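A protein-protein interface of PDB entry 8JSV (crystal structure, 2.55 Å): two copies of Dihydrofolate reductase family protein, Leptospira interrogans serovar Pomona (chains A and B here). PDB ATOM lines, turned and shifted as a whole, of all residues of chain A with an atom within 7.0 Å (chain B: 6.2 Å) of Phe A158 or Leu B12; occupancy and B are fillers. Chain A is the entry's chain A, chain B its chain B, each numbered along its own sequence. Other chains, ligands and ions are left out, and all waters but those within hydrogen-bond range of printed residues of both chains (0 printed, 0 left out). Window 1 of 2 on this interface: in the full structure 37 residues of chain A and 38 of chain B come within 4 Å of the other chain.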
ATOM      1  N   ILE A  10       1.701  10.559 -13.109  1.00  0.00           N
ATOM      2  CA  ILE A  10       2.857   9.908 -13.717  1.00  0.00           C
ATOM      3  C   ILE A  10       2.463   9.175 -14.986  1.00  0.00           C
ATOM      4  O   ILE A  10       1.321   8.736 -15.175  1.00  0.00           O
ATOM      5  CB  ILE A  10       3.604   8.930 -12.772  1.00  0.00           C
ATOM      6  CG1 ILE A  10       2.643   7.919 -12.162  1.00  0.00           C
ATOM      7  CG2 ILE A  10       4.355   9.686 -11.682  1.00  0.00           C
ATOM      8  CD1 ILE A  10       3.266   7.147 -11.043  1.00  0.00           C
ATOM      9  N   LEU A  12       3.280   5.845 -17.570  1.00  0.00           N
ATOM     10  CA  LEU A  12       3.428   4.419 -17.302  1.00  0.00           C
ATOM     11  C   LEU A  12       4.831   4.100 -16.805  1.00  0.00           C
ATOM     12  O   LEU A  12       5.005   3.293 -15.885  1.00  0.00           O
ATOM     13  CB  LEU A  12       3.108   3.608 -18.556  1.00  0.00           C
ATOM     14  CG  LEU A  12       1.634   3.272 -18.728  1.00  0.00           C
ATOM     15  CD1 LEU A  12       1.455   2.453 -19.998  1.00  0.00           C
ATOM     16  CD2 LEU A  12       1.101   2.546 -17.504  1.00  0.00           C
ATOM     17  N   GLY A  14       6.652   6.037 -15.085  1.00  0.00           N
ATOM     18  CA  GLY A  14       6.900   6.841 -13.896  1.00  0.00           C
ATOM     19  C   GLY A  14       7.564   8.196 -14.076  1.00  0.00           C
ATOM     20  O   GLY A  14       8.306   8.623 -13.189  1.00  0.00           O
ATOM     21  N   MET A  16       7.317  12.293 -14.204  1.00  0.00           N
ATOM     22  CA  MET A  16       6.388  13.202 -13.555  1.00  0.00           C
ATOM     23  C   MET A  16       6.595  14.674 -13.990  1.00  0.00           C
ATOM     24  O   MET A  16       5.785  15.557 -13.675  1.00  0.00           O
ATOM     25  CB  MET A  16       6.518  13.027 -12.039  1.00  0.00           C
ATOM     26  CG  MET A  16       7.908  13.364 -11.525  1.00  0.00           C
ATOM     27  SD  MET A  16       8.008  15.208 -10.828  1.00  0.00           S
ATOM     28  CE  MET A  16       6.790  14.891  -9.334  1.00  0.00           C
ATOM     29  N   ILE A 130      10.440  15.206  -2.772  1.00  0.00           N
ATOM     30  CA  ILE A 130       9.871  13.887  -2.532  1.00  0.00           C
ATOM     31  C   ILE A 130      10.970  12.848  -2.369  1.00  0.00           C
ATOM     32  O   ILE A 130      10.813  11.902  -1.590  1.00  0.00           O
ATOM     33  CB  ILE A 130       8.903  13.499  -3.657  1.00  0.00           C
ATOM     34  CG1 ILE A 130       7.553  14.151  -3.417  1.00  0.00           C
ATOM     35  CG2 ILE A 130       8.732  11.987  -3.719  1.00  0.00           C
ATOM     36  CD1 ILE A 130       6.611  13.962  -4.554  1.00  0.00           C
ATOM     37  N   GLN A 131      12.087  12.983  -3.099  1.00  0.00           N
ATOM     38  CA  GLN A 131      13.196  12.047  -2.892  1.00  0.00           C
ATOM     39  C   GLN A 131      13.620  12.001  -1.417  1.00  0.00           C
ATOM     40  O   GLN A 131      13.751  10.923  -0.821  1.00  0.00           O
ATOM     41  CB  GLN A 131      14.382  12.415  -3.786  1.00  0.00           C
ATOM     42  CG  GLN A 131      14.199  12.076  -5.271  1.00  0.00           C
ATOM     43  CD  GLN A 131      13.096  11.071  -5.498  1.00  0.00           C
ATOM     44  OE1 GLN A 131      13.290   9.870  -5.303  1.00  0.00           O
ATOM     45  NE2 GLN A 131      11.922  11.552  -5.893  1.00  0.00           N
ATOM     46  N   PHE A 134      10.830  10.375   0.774  1.00  0.00           N
ATOM     47  CA  PHE A 134      10.860   8.916   0.618  1.00  0.00           C
ATOM     48  C   PHE A 134      12.020   8.293   1.385  1.00  0.00           C
ATOM     49  O   PHE A 134      11.855   7.276   2.066  1.00  0.00           O
ATOM     50  CB  PHE A 134      10.997   8.549  -0.863  1.00  0.00           C
ATOM     51  CG  PHE A 134       9.696   8.487  -1.607  1.00  0.00           C
ATOM     52  CD1 PHE A 134       8.500   8.340  -0.935  1.00  0.00           C
ATOM     53  CD2 PHE A 134       9.684   8.560  -2.996  1.00  0.00           C
ATOM     54  CE1 PHE A 134       7.305   8.273  -1.624  1.00  0.00           C
ATOM     55  CE2 PHE A 134       8.496   8.490  -3.700  1.00  0.00           C
ATOM     56  CZ  PHE A 134       7.299   8.341  -3.010  1.00  0.00           C
ATOM     57  N   LEU A 142      -0.027   7.744  -0.790  1.00  0.00           N
ATOM     58  CA  LEU A 142       0.228   8.065  -2.191  1.00  0.00           C
ATOM     59  C   LEU A 142      -1.087   8.101  -2.954  1.00  0.00           C
ATOM     60  O   LEU A 142      -1.764   7.079  -3.059  1.00  0.00           O
ATOM     61  CB  LEU A 142       1.143   7.029  -2.836  1.00  0.00           C
ATOM     62  CG  LEU A 142       2.630   6.979  -2.539  1.00  0.00           C
ATOM     63  CD1 LEU A 142       3.335   6.434  -3.764  1.00  0.00           C
ATOM     64  CD2 LEU A 142       3.125   8.348  -2.224  1.00  0.00           C
ATOM     65  N   LEU A 144      -2.059   8.584  -6.755  1.00  0.00           N
ATOM     66  CA  LEU A 144      -1.395   8.571  -8.036  1.00  0.00           C
ATOM     67  C   LEU A 144      -2.442   8.592  -9.132  1.00  0.00           C
ATOM     68  O   LEU A 144      -3.548   8.065  -8.970  1.00  0.00           O
ATOM     69  CB  LEU A 144      -0.513   7.323  -8.196  1.00  0.00           C
ATOM     70  CG  LEU A 144       0.617   7.088  -7.194  1.00  0.00           C
ATOM     71  CD1 LEU A 144       1.317   5.757  -7.477  1.00  0.00           C
ATOM     72  CD2 LEU A 144       1.614   8.221  -7.254  1.00  0.00           C
ATOM     73  N   ILE A 146      -2.100   7.423 -13.116  1.00  0.00           N
ATOM     74  CA  ILE A 146      -1.218   6.827 -14.113  1.00  0.00           C
ATOM     75  C   ILE A 146      -1.868   6.969 -15.483  1.00  0.00           C
ATOM     76  O   ILE A 146      -3.020   6.556 -15.684  1.00  0.00           O
ATOM     77  CB  ILE A 146      -0.894   5.357 -13.780  1.00  0.00           C
ATOM     78  CG1 ILE A 146      -0.278   5.271 -12.385  1.00  0.00           C
ATOM     79  CG2 ILE A 146       0.127   4.805 -14.771  1.00  0.00           C
ATOM     80  CD1 ILE A 146      -1.262   4.912 -11.281  1.00  0.00           C
ATOM     81  N   LYS A 155      12.022  13.918 -15.287  1.00  0.00           N
ATOM     82  CA  LYS A 155      12.169  13.724 -13.825  1.00  0.00           C
ATOM     83  C   LYS A 155      11.203  12.621 -13.403  1.00  0.00           C
ATOM     84  O   LYS A 155      10.123  12.533 -13.991  1.00  0.00           O
ATOM     85  CB  LYS A 155      11.958  15.042 -13.078  1.00  0.00           C
ATOM     86  CG  LYS A 155      13.023  16.103 -13.313  1.00  0.00           C
ATOM     87  CD  LYS A 155      12.553  17.497 -12.975  1.00  0.00           C
ATOM     88  CE  LYS A 155      13.668  18.518 -13.020  1.00  0.00           C
ATOM     89  NZ  LYS A 155      13.208  19.853 -12.571  1.00  0.00           N
ATOM     90  N   ARG A 156      11.569  11.838 -12.391  1.00  0.00           N
ATOM     91  CA  ARG A 156      10.753  10.675 -12.053  1.00  0.00           C
ATOM     92  C   ARG A 156      10.217  10.781 -10.632  1.00  0.00           C
ATOM     93  O   ARG A 156      10.818  11.425  -9.774  1.00  0.00           O
ATOM     94  CB  ARG A 156      11.551   9.377 -12.221  1.00  0.00           C
ATOM     95  CG  ARG A 156      12.005   9.137 -13.647  1.00  0.00           C
ATOM     96  CD  ARG A 156      12.676   7.766 -13.863  1.00  0.00           C
ATOM     97  NE  ARG A 156      11.675   6.721 -14.042  1.00  0.00           N
ATOM     98  CZ  ARG A 156      11.180   5.979 -13.054  1.00  0.00           C
ATOM     99  NH1 ARG A 156      11.711   5.996 -11.835  1.00  0.00           N
ATOM    100  NH2 ARG A 156      10.131   5.192 -13.294  1.00  0.00           N
ATOM    101  N   LEU A 157       9.064  10.160 -10.382  1.00  0.00           N
ATOM    102  CA  LEU A 157       8.508  10.194  -9.032  1.00  0.00           C
ATOM    103  C   LEU A 157       9.278   9.269  -8.094  1.00  0.00           C
ATOM    104  O   LEU A 157       9.729   9.682  -7.021  1.00  0.00           O
ATOM    105  CB  LEU A 157       7.046   9.814  -9.073  1.00  0.00           C
ATOM    106  CG  LEU A 157       6.501   9.395  -7.733  1.00  0.00           C
ATOM    107  CD1 LEU A 157       6.495  10.591  -6.775  1.00  0.00           C
ATOM    108  CD2 LEU A 157       5.104   8.850  -7.968  1.00  0.00           C
ATOM    109  N   PHE A 158       9.467   8.018  -8.496  1.00  0.00           N
ATOM    110  CA  PHE A 158      10.330   7.099  -7.756  1.00  0.00           C
ATOM    111  C   PHE A 158      11.744   7.243  -8.295  1.00  0.00           C
ATOM    112  O   PHE A 158      12.147   6.551  -9.242  1.00  0.00           O
ATOM    113  CB  PHE A 158       9.826   5.675  -7.879  1.00  0.00           C
ATOM    114  CG  PHE A 158       8.441   5.503  -7.373  1.00  0.00           C
ATOM    115  CD1 PHE A 158       8.162   5.707  -6.043  1.00  0.00           C
ATOM    116  CD2 PHE A 158       7.403   5.167  -8.239  1.00  0.00           C
ATOM    117  CE1 PHE A 158       6.871   5.562  -5.565  1.00  0.00           C
ATOM    118  CE2 PHE A 158       6.101   5.007  -7.776  1.00  0.00           C
ATOM    119  CZ  PHE A 158       5.830   5.204  -6.438  1.00  0.00           C
ATOM    120  N   GLY A 159      12.505   8.151  -7.674  1.00  0.00           N
ATOM    121  CA  GLY A 159      13.869   8.409  -8.086  1.00  0.00           C
ATOM    122  C   GLY A 159      14.898   8.040  -7.039  1.00  0.00           C
ATOM    123  O   GLY A 159      14.765   7.021  -6.362  1.00  0.00           O
ATOM    124  N   ASP A 160      15.891   8.919  -6.875  1.00  0.00           N
ATOM    125  CA  ASP A 160      17.061   8.668  -6.038  1.00  0.00           C
ATOM    126  C   ASP A 160      16.716   8.202  -4.630  1.00  0.00           C
ATOM    127  O   ASP A 160      17.446   7.398  -4.040  1.00  0.00           O
ATOM    128  CB  ASP A 160      17.883   9.946  -5.937  1.00  0.00           C
ATOM    129  CG  ASP A 160      19.085   9.917  -6.810  1.00  0.00           C
ATOM    130  OD1 ASP A 160      19.430   8.812  -7.291  1.00  0.00           O
ATOM    131  OD2 ASP A 160      19.684  10.999  -7.016  1.00  0.00           O
ATOM    132  N   GLY A 161      15.658   8.743  -4.047  1.00  0.00           N
ATOM    133  CA  GLY A 161      15.370   8.459  -2.661  1.00  0.00           C
ATOM    134  C   GLY A 161      14.429   7.313  -2.419  1.00  0.00           C
ATOM    135  O   GLY A 161      14.154   6.996  -1.259  1.00  0.00           O
ATOM    136  N   THR A 162      13.920   6.688  -3.477  1.00  0.00           N
ATOM    137  CA  THR A 162      13.055   5.525  -3.341  1.00  0.00           C
ATOM    138  C   THR A 162      13.735   4.453  -2.498  1.00  0.00           C
ATOM    139  O   THR A 162      14.914   4.128  -2.700  1.00  0.00           O
ATOM    140  CB  THR A 162      12.713   4.952  -4.724  1.00  0.00           C
ATOM    141  OG1 THR A 162      12.752   5.993  -5.715  1.00  0.00           O
ATOM    142  CG2 THR A 162      11.351   4.289  -4.719  1.00  0.00           C
ATOM    143  N   ILE A 163      12.986   3.924  -1.540  1.00  0.00           N
ATOM    144  CA  ILE A 163      13.467   2.878  -0.641  1.00  0.00           C
ATOM    145  C   ILE A 163      12.609   1.651  -0.894  1.00  0.00           C
ATOM    146  O   ILE A 163      11.549   1.751  -1.527  1.00  0.00           O
ATOM    147  CB  ILE A 163      13.393   3.312   0.841  1.00  0.00           C
ATOM    148  CG1 ILE A 163      11.924   3.489   1.240  1.00  0.00           C
ATOM    149  CG2 ILE A 163      14.215   4.565   1.054  1.00  0.00           C
ATOM    150  CD1 ILE A 163      11.633   3.229   2.728  1.00  0.00           C
ATOM    151  N   ALA A 165       9.798  -0.669   0.095  1.00  0.00           N
ATOM    152  CA  ALA A 165       8.653  -0.465   0.977  1.00  0.00           C
ATOM    153  C   ALA A 165       7.402  -1.122   0.399  1.00  0.00           C
ATOM    154  O   ALA A 165       7.291  -1.346  -0.808  1.00  0.00           O
ATOM    155  CB  ALA A 165       8.408   1.031   1.215  1.00  0.00           C
ATOM    156  N   PHE A 167       2.933  -1.329   0.373  1.00  0.00           N
ATOM    157  CA  PHE A 167       1.744  -0.486   0.431  1.00  0.00           C
ATOM    158  C   PHE A 167       0.481  -1.338   0.344  1.00  0.00           C
ATOM    159  O   PHE A 167       0.503  -2.479  -0.112  1.00  0.00           O
ATOM    160  CB  PHE A 167       1.727   0.564  -0.701  1.00  0.00           C
ATOM    161  CG  PHE A 167       2.912   1.487  -0.690  1.00  0.00           C
ATOM    162  CD1 PHE A 167       2.900   2.637   0.071  1.00  0.00           C
ATOM    163  CD2 PHE A 167       4.050   1.190  -1.430  1.00  0.00           C
ATOM    164  CE1 PHE A 167       3.985   3.474   0.087  1.00  0.00           C
ATOM    165  CE2 PHE A 167       5.141   2.027  -1.413  1.00  0.00           C
ATOM    166  CZ  PHE A 167       5.104   3.170  -0.651  1.00  0.00           C
ATOM    167  N   ALA A 182      -4.919   5.549  -8.415  1.00  0.00           N
ATOM    168  CA  ALA A 182      -4.482   4.529  -7.470  1.00  0.00           C
ATOM    169  C   ALA A 182      -4.106   5.168  -6.153  1.00  0.00           C
ATOM    170  O   ALA A 182      -3.350   6.139  -6.122  1.00  0.00           O
ATOM    171  CB  ALA A 182      -3.302   3.740  -8.023  1.00  0.00           C
ATOM    172  N   TYR A 184      -2.572   4.472  -2.474  1.00  0.00           N
ATOM    173  CA  TYR A 184      -1.844   3.559  -1.605  1.00  0.00           C
ATOM    174  C   TYR A 184      -1.629   4.129  -0.207  1.00  0.00           C
ATOM    175  O   TYR A 184      -1.482   5.338  -0.020  1.00  0.00           O
ATOM    176  CB  TYR A 184      -0.497   3.199  -2.224  1.00  0.00           C
ATOM    177  CG  TYR A 184      -0.654   2.542  -3.555  1.00  0.00           C
ATOM    178  CD1 TYR A 184      -0.824   1.166  -3.663  1.00  0.00           C
ATOM    179  CD2 TYR A 184      -0.675   3.293  -4.706  1.00  0.00           C
ATOM    180  CE1 TYR A 184      -0.983   0.558  -4.900  1.00  0.00           C
ATOM    181  CE2 TYR A 184      -0.829   2.699  -5.939  1.00  0.00           C
ATOM    182  CZ  TYR A 184      -0.980   1.334  -6.038  1.00  0.00           C
ATOM    183  OH  TYR A 184      -1.141   0.771  -7.294  1.00  0.00           O
ATOM    184  N   ILE B  10       5.231  -5.859 -12.516  1.00  0.00           N
ATOM    185  CA  ILE B  10       6.102  -4.746 -12.160  1.00  0.00           C
ATOM    186  C   ILE B  10       5.683  -4.222 -10.806  1.00  0.00           C
ATOM    187  O   ILE B  10       4.529  -4.371 -10.394  1.00  0.00           O
ATOM    188  CB  ILE B  10       6.052  -3.617 -13.200  1.00  0.00           C
ATOM    189  CG1 ILE B  10       4.611  -3.123 -13.345  1.00  0.00           C
ATOM    190  CG2 ILE B  10       6.611  -4.097 -14.537  1.00  0.00           C
ATOM    191  CD1 ILE B  10       4.357  -2.388 -14.638  1.00  0.00           C
ATOM    192  N   THR B  11       6.642  -3.628 -10.098  1.00  0.00           N
ATOM    193  CA  THR B  11       6.348  -2.919  -8.863  1.00  0.00           C
ATOM    194  C   THR B  11       5.742  -1.554  -9.185  1.00  0.00           C
ATOM    195  O   THR B  11       5.600  -1.167 -10.351  1.00  0.00           O
ATOM    196  CB  THR B  11       7.613  -2.767  -8.030  1.00  0.00           C
ATOM    197  OG1 THR B  11       8.607  -2.091  -8.812  1.00  0.00           O
ATOM    198  CG2 THR B  11       8.137  -4.124  -7.643  1.00  0.00           C
ATOM    199  N   LEU B  12       5.392  -0.799  -8.139  1.00  0.00           N
ATOM    200  CA  LEU B  12       4.940   0.576  -8.351  1.00  0.00           C
ATOM    201  C   LEU B  12       6.005   1.421  -9.043  1.00  0.00           C
ATOM    202  O   LEU B  12       5.666   2.294  -9.848  1.00  0.00           O
ATOM    203  CB  LEU B  12       4.544   1.221  -7.027  1.00  0.00           C
ATOM    204  CG  LEU B  12       3.120   1.000  -6.518  1.00  0.00           C
ATOM    205  CD1 LEU B  12       2.926   1.754  -5.208  1.00  0.00           C
ATOM    206  CD2 LEU B  12       2.095   1.430  -7.543  1.00  0.00           C
ATOM    207  N   ASP B  13       7.290   1.182  -8.766  1.00  0.00           N
ATOM    208  CA  ASP B  13       8.350   1.893  -9.470  1.00  0.00           C
ATOM    209  C   ASP B  13       8.872   1.135 -10.681  1.00  0.00           C
ATOM    210  O   ASP B  13       9.940   1.479 -11.202  1.00  0.00           O
ATOM    211  CB  ASP B  13       9.493   2.264  -8.516  1.00  0.00           C
ATOM    212  CG  ASP B  13      10.196   1.059  -7.890  1.00  0.00           C
ATOM    213  OD1 ASP B  13       9.519   0.123  -7.399  1.00  0.00           O
ATOM    214  OD2 ASP B  13      11.451   1.093  -7.825  1.00  0.00           O
ATOM    215  N   GLY B  14       8.145   0.118 -11.146  1.00  0.00           N
ATOM    216  CA  GLY B  14       8.434  -0.483 -12.434  1.00  0.00           C
ATOM    217  C   GLY B  14       9.568  -1.475 -12.502  1.00  0.00           C
ATOM    218  O   GLY B  14      10.122  -1.674 -13.584  1.00  0.00           O
ATOM    219  N   VAL B  15       9.942  -2.112 -11.396  1.00  0.00           N
ATOM    220  CA  VAL B  15      10.939  -3.181 -11.443  1.00  0.00           C
ATOM    221  C   VAL B  15      10.256  -4.489 -11.822  1.00  0.00           C
ATOM    222  O   VAL B  15       9.199  -4.833 -11.279  1.00  0.00           O
ATOM    223  CB  VAL B  15      11.660  -3.318 -10.095  1.00  0.00           C
ATOM    224  CG1 VAL B  15      12.618  -4.486 -10.142  1.00  0.00           C
ATOM    225  CG2 VAL B  15      12.386  -2.036  -9.749  1.00  0.00           C
ATOM    226  N   ILE B 146       0.451  -4.505 -11.599  1.00  0.00           N
ATOM    227  CA  ILE B 146       1.181  -3.535 -10.801  1.00  0.00           C
ATOM    228  C   ILE B 146       0.989  -3.892  -9.341  1.00  0.00           C
ATOM    229  O   ILE B 146      -0.147  -3.976  -8.852  1.00  0.00           O
ATOM    230  CB  ILE B 146       0.698  -2.110 -11.088  1.00  0.00           C
ATOM    231  CG1 ILE B 146       0.543  -1.930 -12.587  1.00  0.00           C
ATOM    232  CG2 ILE B 146       1.667  -1.092 -10.512  1.00  0.00           C
ATOM    233  CD1 ILE B 146       0.551  -0.521 -13.012  1.00  0.00           C
ATOM    234  N   PHE B 147       2.096  -4.087  -8.655  1.00  0.00           N
ATOM    235  CA  PHE B 147       2.049  -4.612  -7.313  1.00  0.00           C
ATOM    236  C   PHE B 147       2.323  -3.521  -6.285  1.00  0.00           C
ATOM    237  O   PHE B 147       3.211  -2.682  -6.483  1.00  0.00           O
ATOM    238  CB  PHE B 147       3.064  -5.760  -7.149  1.00  0.00           C
ATOM    239  CG  PHE B 147       2.645  -7.040  -7.847  1.00  0.00           C
ATOM    240  CD1 PHE B 147       2.764  -7.170  -9.229  1.00  0.00           C
ATOM    241  CD2 PHE B 147       2.096  -8.096  -7.126  1.00  0.00           C
ATOM    242  CE1 PHE B 147       2.360  -8.343  -9.876  1.00  0.00           C
ATOM    243  CE2 PHE B 147       1.678  -9.273  -7.772  1.00  0.00           C
ATOM    244  CZ  PHE B 147       1.815  -9.392  -9.143  1.00  0.00           C
ATOM    245  N   PRO B 148       1.597  -3.535  -5.168  1.00  0.00           N
ATOM    246  CA  PRO B 148       1.659  -2.419  -4.213  1.00  0.00           C
ATOM    247  C   PRO B 148       2.952  -2.346  -3.417  1.00  0.00           C
ATOM    248  O   PRO B 148       2.938  -2.221  -2.185  1.00  0.00           O
ATOM    249  CB  PRO B 148       0.473  -2.700  -3.287  1.00  0.00           C
ATOM    250  CG  PRO B 148       0.308  -4.175  -3.338  1.00  0.00           C
ATOM    251  CD  PRO B 148       0.669  -4.591  -4.738  1.00  0.00           C
ATOM    252  N   VAL B 149       4.073  -2.389  -4.133  1.00  0.00           N
ATOM    253  CA  VAL B 149       5.391  -2.441  -3.447  1.00  0.00           C
ATOM    254  C   VAL B 149       6.393  -1.581  -4.215  1.00  0.00           C
ATOM    255  O   VAL B 149       6.189  -1.376  -5.414  1.00  0.00           O
ATOM    256  CB  VAL B 149       5.858  -3.905  -3.357  1.00  0.00           C
ATOM    257  CG1 VAL B 149       5.790  -4.609  -4.701  1.00  0.00           C
ATOM    258  CG2 VAL B 149       7.236  -4.059  -2.740  1.00  0.00           C
ATOM    259  N   THR B 150       7.412  -1.069  -3.528  1.00  0.00           N
ATOM    260  CA  THR B 150       8.489  -0.308  -4.206  1.00  0.00           C
ATOM    261  C   THR B 150       9.838  -0.942  -3.860  1.00  0.00           C
ATOM    262  O   THR B 150      10.010  -1.331  -2.701  1.00  0.00           O
ATOM    263  CB  THR B 150       8.432   1.179  -3.846  1.00  0.00           C
ATOM    264  OG1 THR B 150       9.550   1.784  -4.488  1.00  0.00           O
ATOM    265  CG2 THR B 150       8.476   1.453  -2.361  1.00  0.00           C
ATOM    266  N   ARG B 156      14.311  -3.167 -14.930  1.00  0.00           N
ATOM    267  CA  ARG B 156      13.077  -2.413 -15.127  1.00  0.00           C
ATOM    268  C   ARG B 156      12.401  -2.824 -16.427  1.00  0.00           C
ATOM    269  O   ARG B 156      13.071  -3.046 -17.441  1.00  0.00           O
ATOM    270  CB  ARG B 156      13.368  -0.911 -15.140  1.00  0.00           C
ATOM    271  CG  ARG B 156      14.470  -0.482 -14.159  1.00  0.00           C
ATOM    272  CD  ARG B 156      14.585   1.033 -14.067  1.00  0.00           C
ATOM    273  NE  ARG B 156      13.278   1.670 -14.189  1.00  0.00           N
ATOM    274  CZ  ARG B 156      12.450   1.906 -13.179  1.00  0.00           C
ATOM    275  NH1 ARG B 156      12.784   1.629 -11.922  1.00  0.00           N
ATOM    276  NH2 ARG B 156      11.251   2.422 -13.433  1.00  0.00           N
ATOM    277  N   ILE B 180      -3.042  -4.268  -9.488  1.00  0.00           N
ATOM    278  CA  ILE B 180      -3.807  -3.608 -10.532  1.00  0.00           C
ATOM    279  C   ILE B 180      -3.515  -4.293 -11.850  1.00  0.00           C
ATOM    280  O   ILE B 180      -2.376  -4.271 -12.336  1.00  0.00           O
ATOM    281  CB  ILE B 180      -3.487  -2.112 -10.622  1.00  0.00           C
ATOM    282  CG1 ILE B 180      -3.933  -1.411  -9.347  1.00  0.00           C
ATOM    283  CG2 ILE B 180      -4.159  -1.506 -11.861  1.00  0.00           C
ATOM    284  CD1 ILE B 180      -3.538   0.020  -9.312  1.00  0.00           C
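The guanidinium group (NH2) of Arg A156 lies close to the guanidinium group (NH2) of Arg B156 (3.0 Å).
The backbone carbonyl oxygen (O) of Pro B148 sits at hydrogen-bond distance from the backbone NH (N) of Phe A167 (2.7 Å).
O of Ala A165 sits at hydrogen-bond distance from N of Thr B150.
The backbone NH of Leu A144 sits at hydrogen-bond distance from the backbone carbonyl oxygen of Ala A182.
The backbone NH (N) of Ile B146 sits at hydrogen-bond distance from the backbone carbonyl oxygen (O) of Ile B180 (2.9 Å).
N of Tyr A184 sits at hydrogen-bond distance from O of Leu A142 (2.8 Å).
The backbone NH (N) of Leu B12 lies within hydrogen-bond range of the backbone carbonyl oxygen (O) of Val B149 (2.9 Å).
OD1 of Asp B13 sits at hydrogen-bond distance from OG1 of Thr B11, at 2.8 Å.
The backbone NH (N) of Leu B12 lies within hydrogen-bond range of the backbone carbonyl oxygen (O) of Phe B147, 3.3 Å away.
CE2 of Phe A158 touches O of Leu B12, at 3.4 Å.
Phe A158 touches Asp B13.
Thr B150 touches Thr A162 (OG1 to CG2, 3.1 Å).
CG2 of Thr B150 touches O of Ile A163, at 3.2 Å.
CG2 of Val B149 touches O of Ala A165 (3.3 Å).
Phe A167 touches Leu B12 (CD2 to CD1, 3.98 Å).
Phe A167 touches Thr B150 (CE2 to CG2, 3.5 Å).
CB of Ala A182 touches CD1 of Ile B180, 3.9 Å away.
Pro B148 touches Tyr A184.
Tyr A184 touches Ile B180 (OH to CD1, 3.2 Å).
Of chain B, only Leu B12 (3.4 Å) and Asp B13 (3.5 Å) come within 4 Å of Phe A158.
Printed residues of chain A within 4 Å of Leu B12: Phe A158 (3.4 Å), Phe A167 (3.98 Å) and Tyr A184 (3.3 Å).
Of the printed residues of chain B, Arg A156 touches Arg B156.
Printed residues of chain B within 4 Å of Thr A162: Thr B150 (3.1 Å).
Phe B147 touches none of the printed residues of chain A.
Leu A144 touches none of the printed residues of chain B.
The nearest printed residue of chain A that does not touch Leu B12 is Leu A144 (4.4 Å).
Printed residues of chain A that touch a printed residue of chain B: Arg A156, Phe A158, Thr A162, Ile A163, Ala A165, Phe A167, Ala A182 and Tyr A184.
Of the 13 printed residues of chain B, 7 touch a printed residue of chain A.
Printed residues of chain B that touch a printed residue of chain A: Leu B12, Asp B13, Pro B148, Val B149, Thr B150, Arg B156 and Ile B180.
Among the printed residues, 14 pairs touch across the chains.
Among the printed residues, no Asp or Glu carboxylate lies within 4 Å of a Lys or Arg side-chain nitrogen of the other chain.
Arg B156 touches its own counterpart, Arg A156.
5 positions are printed for both chains.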
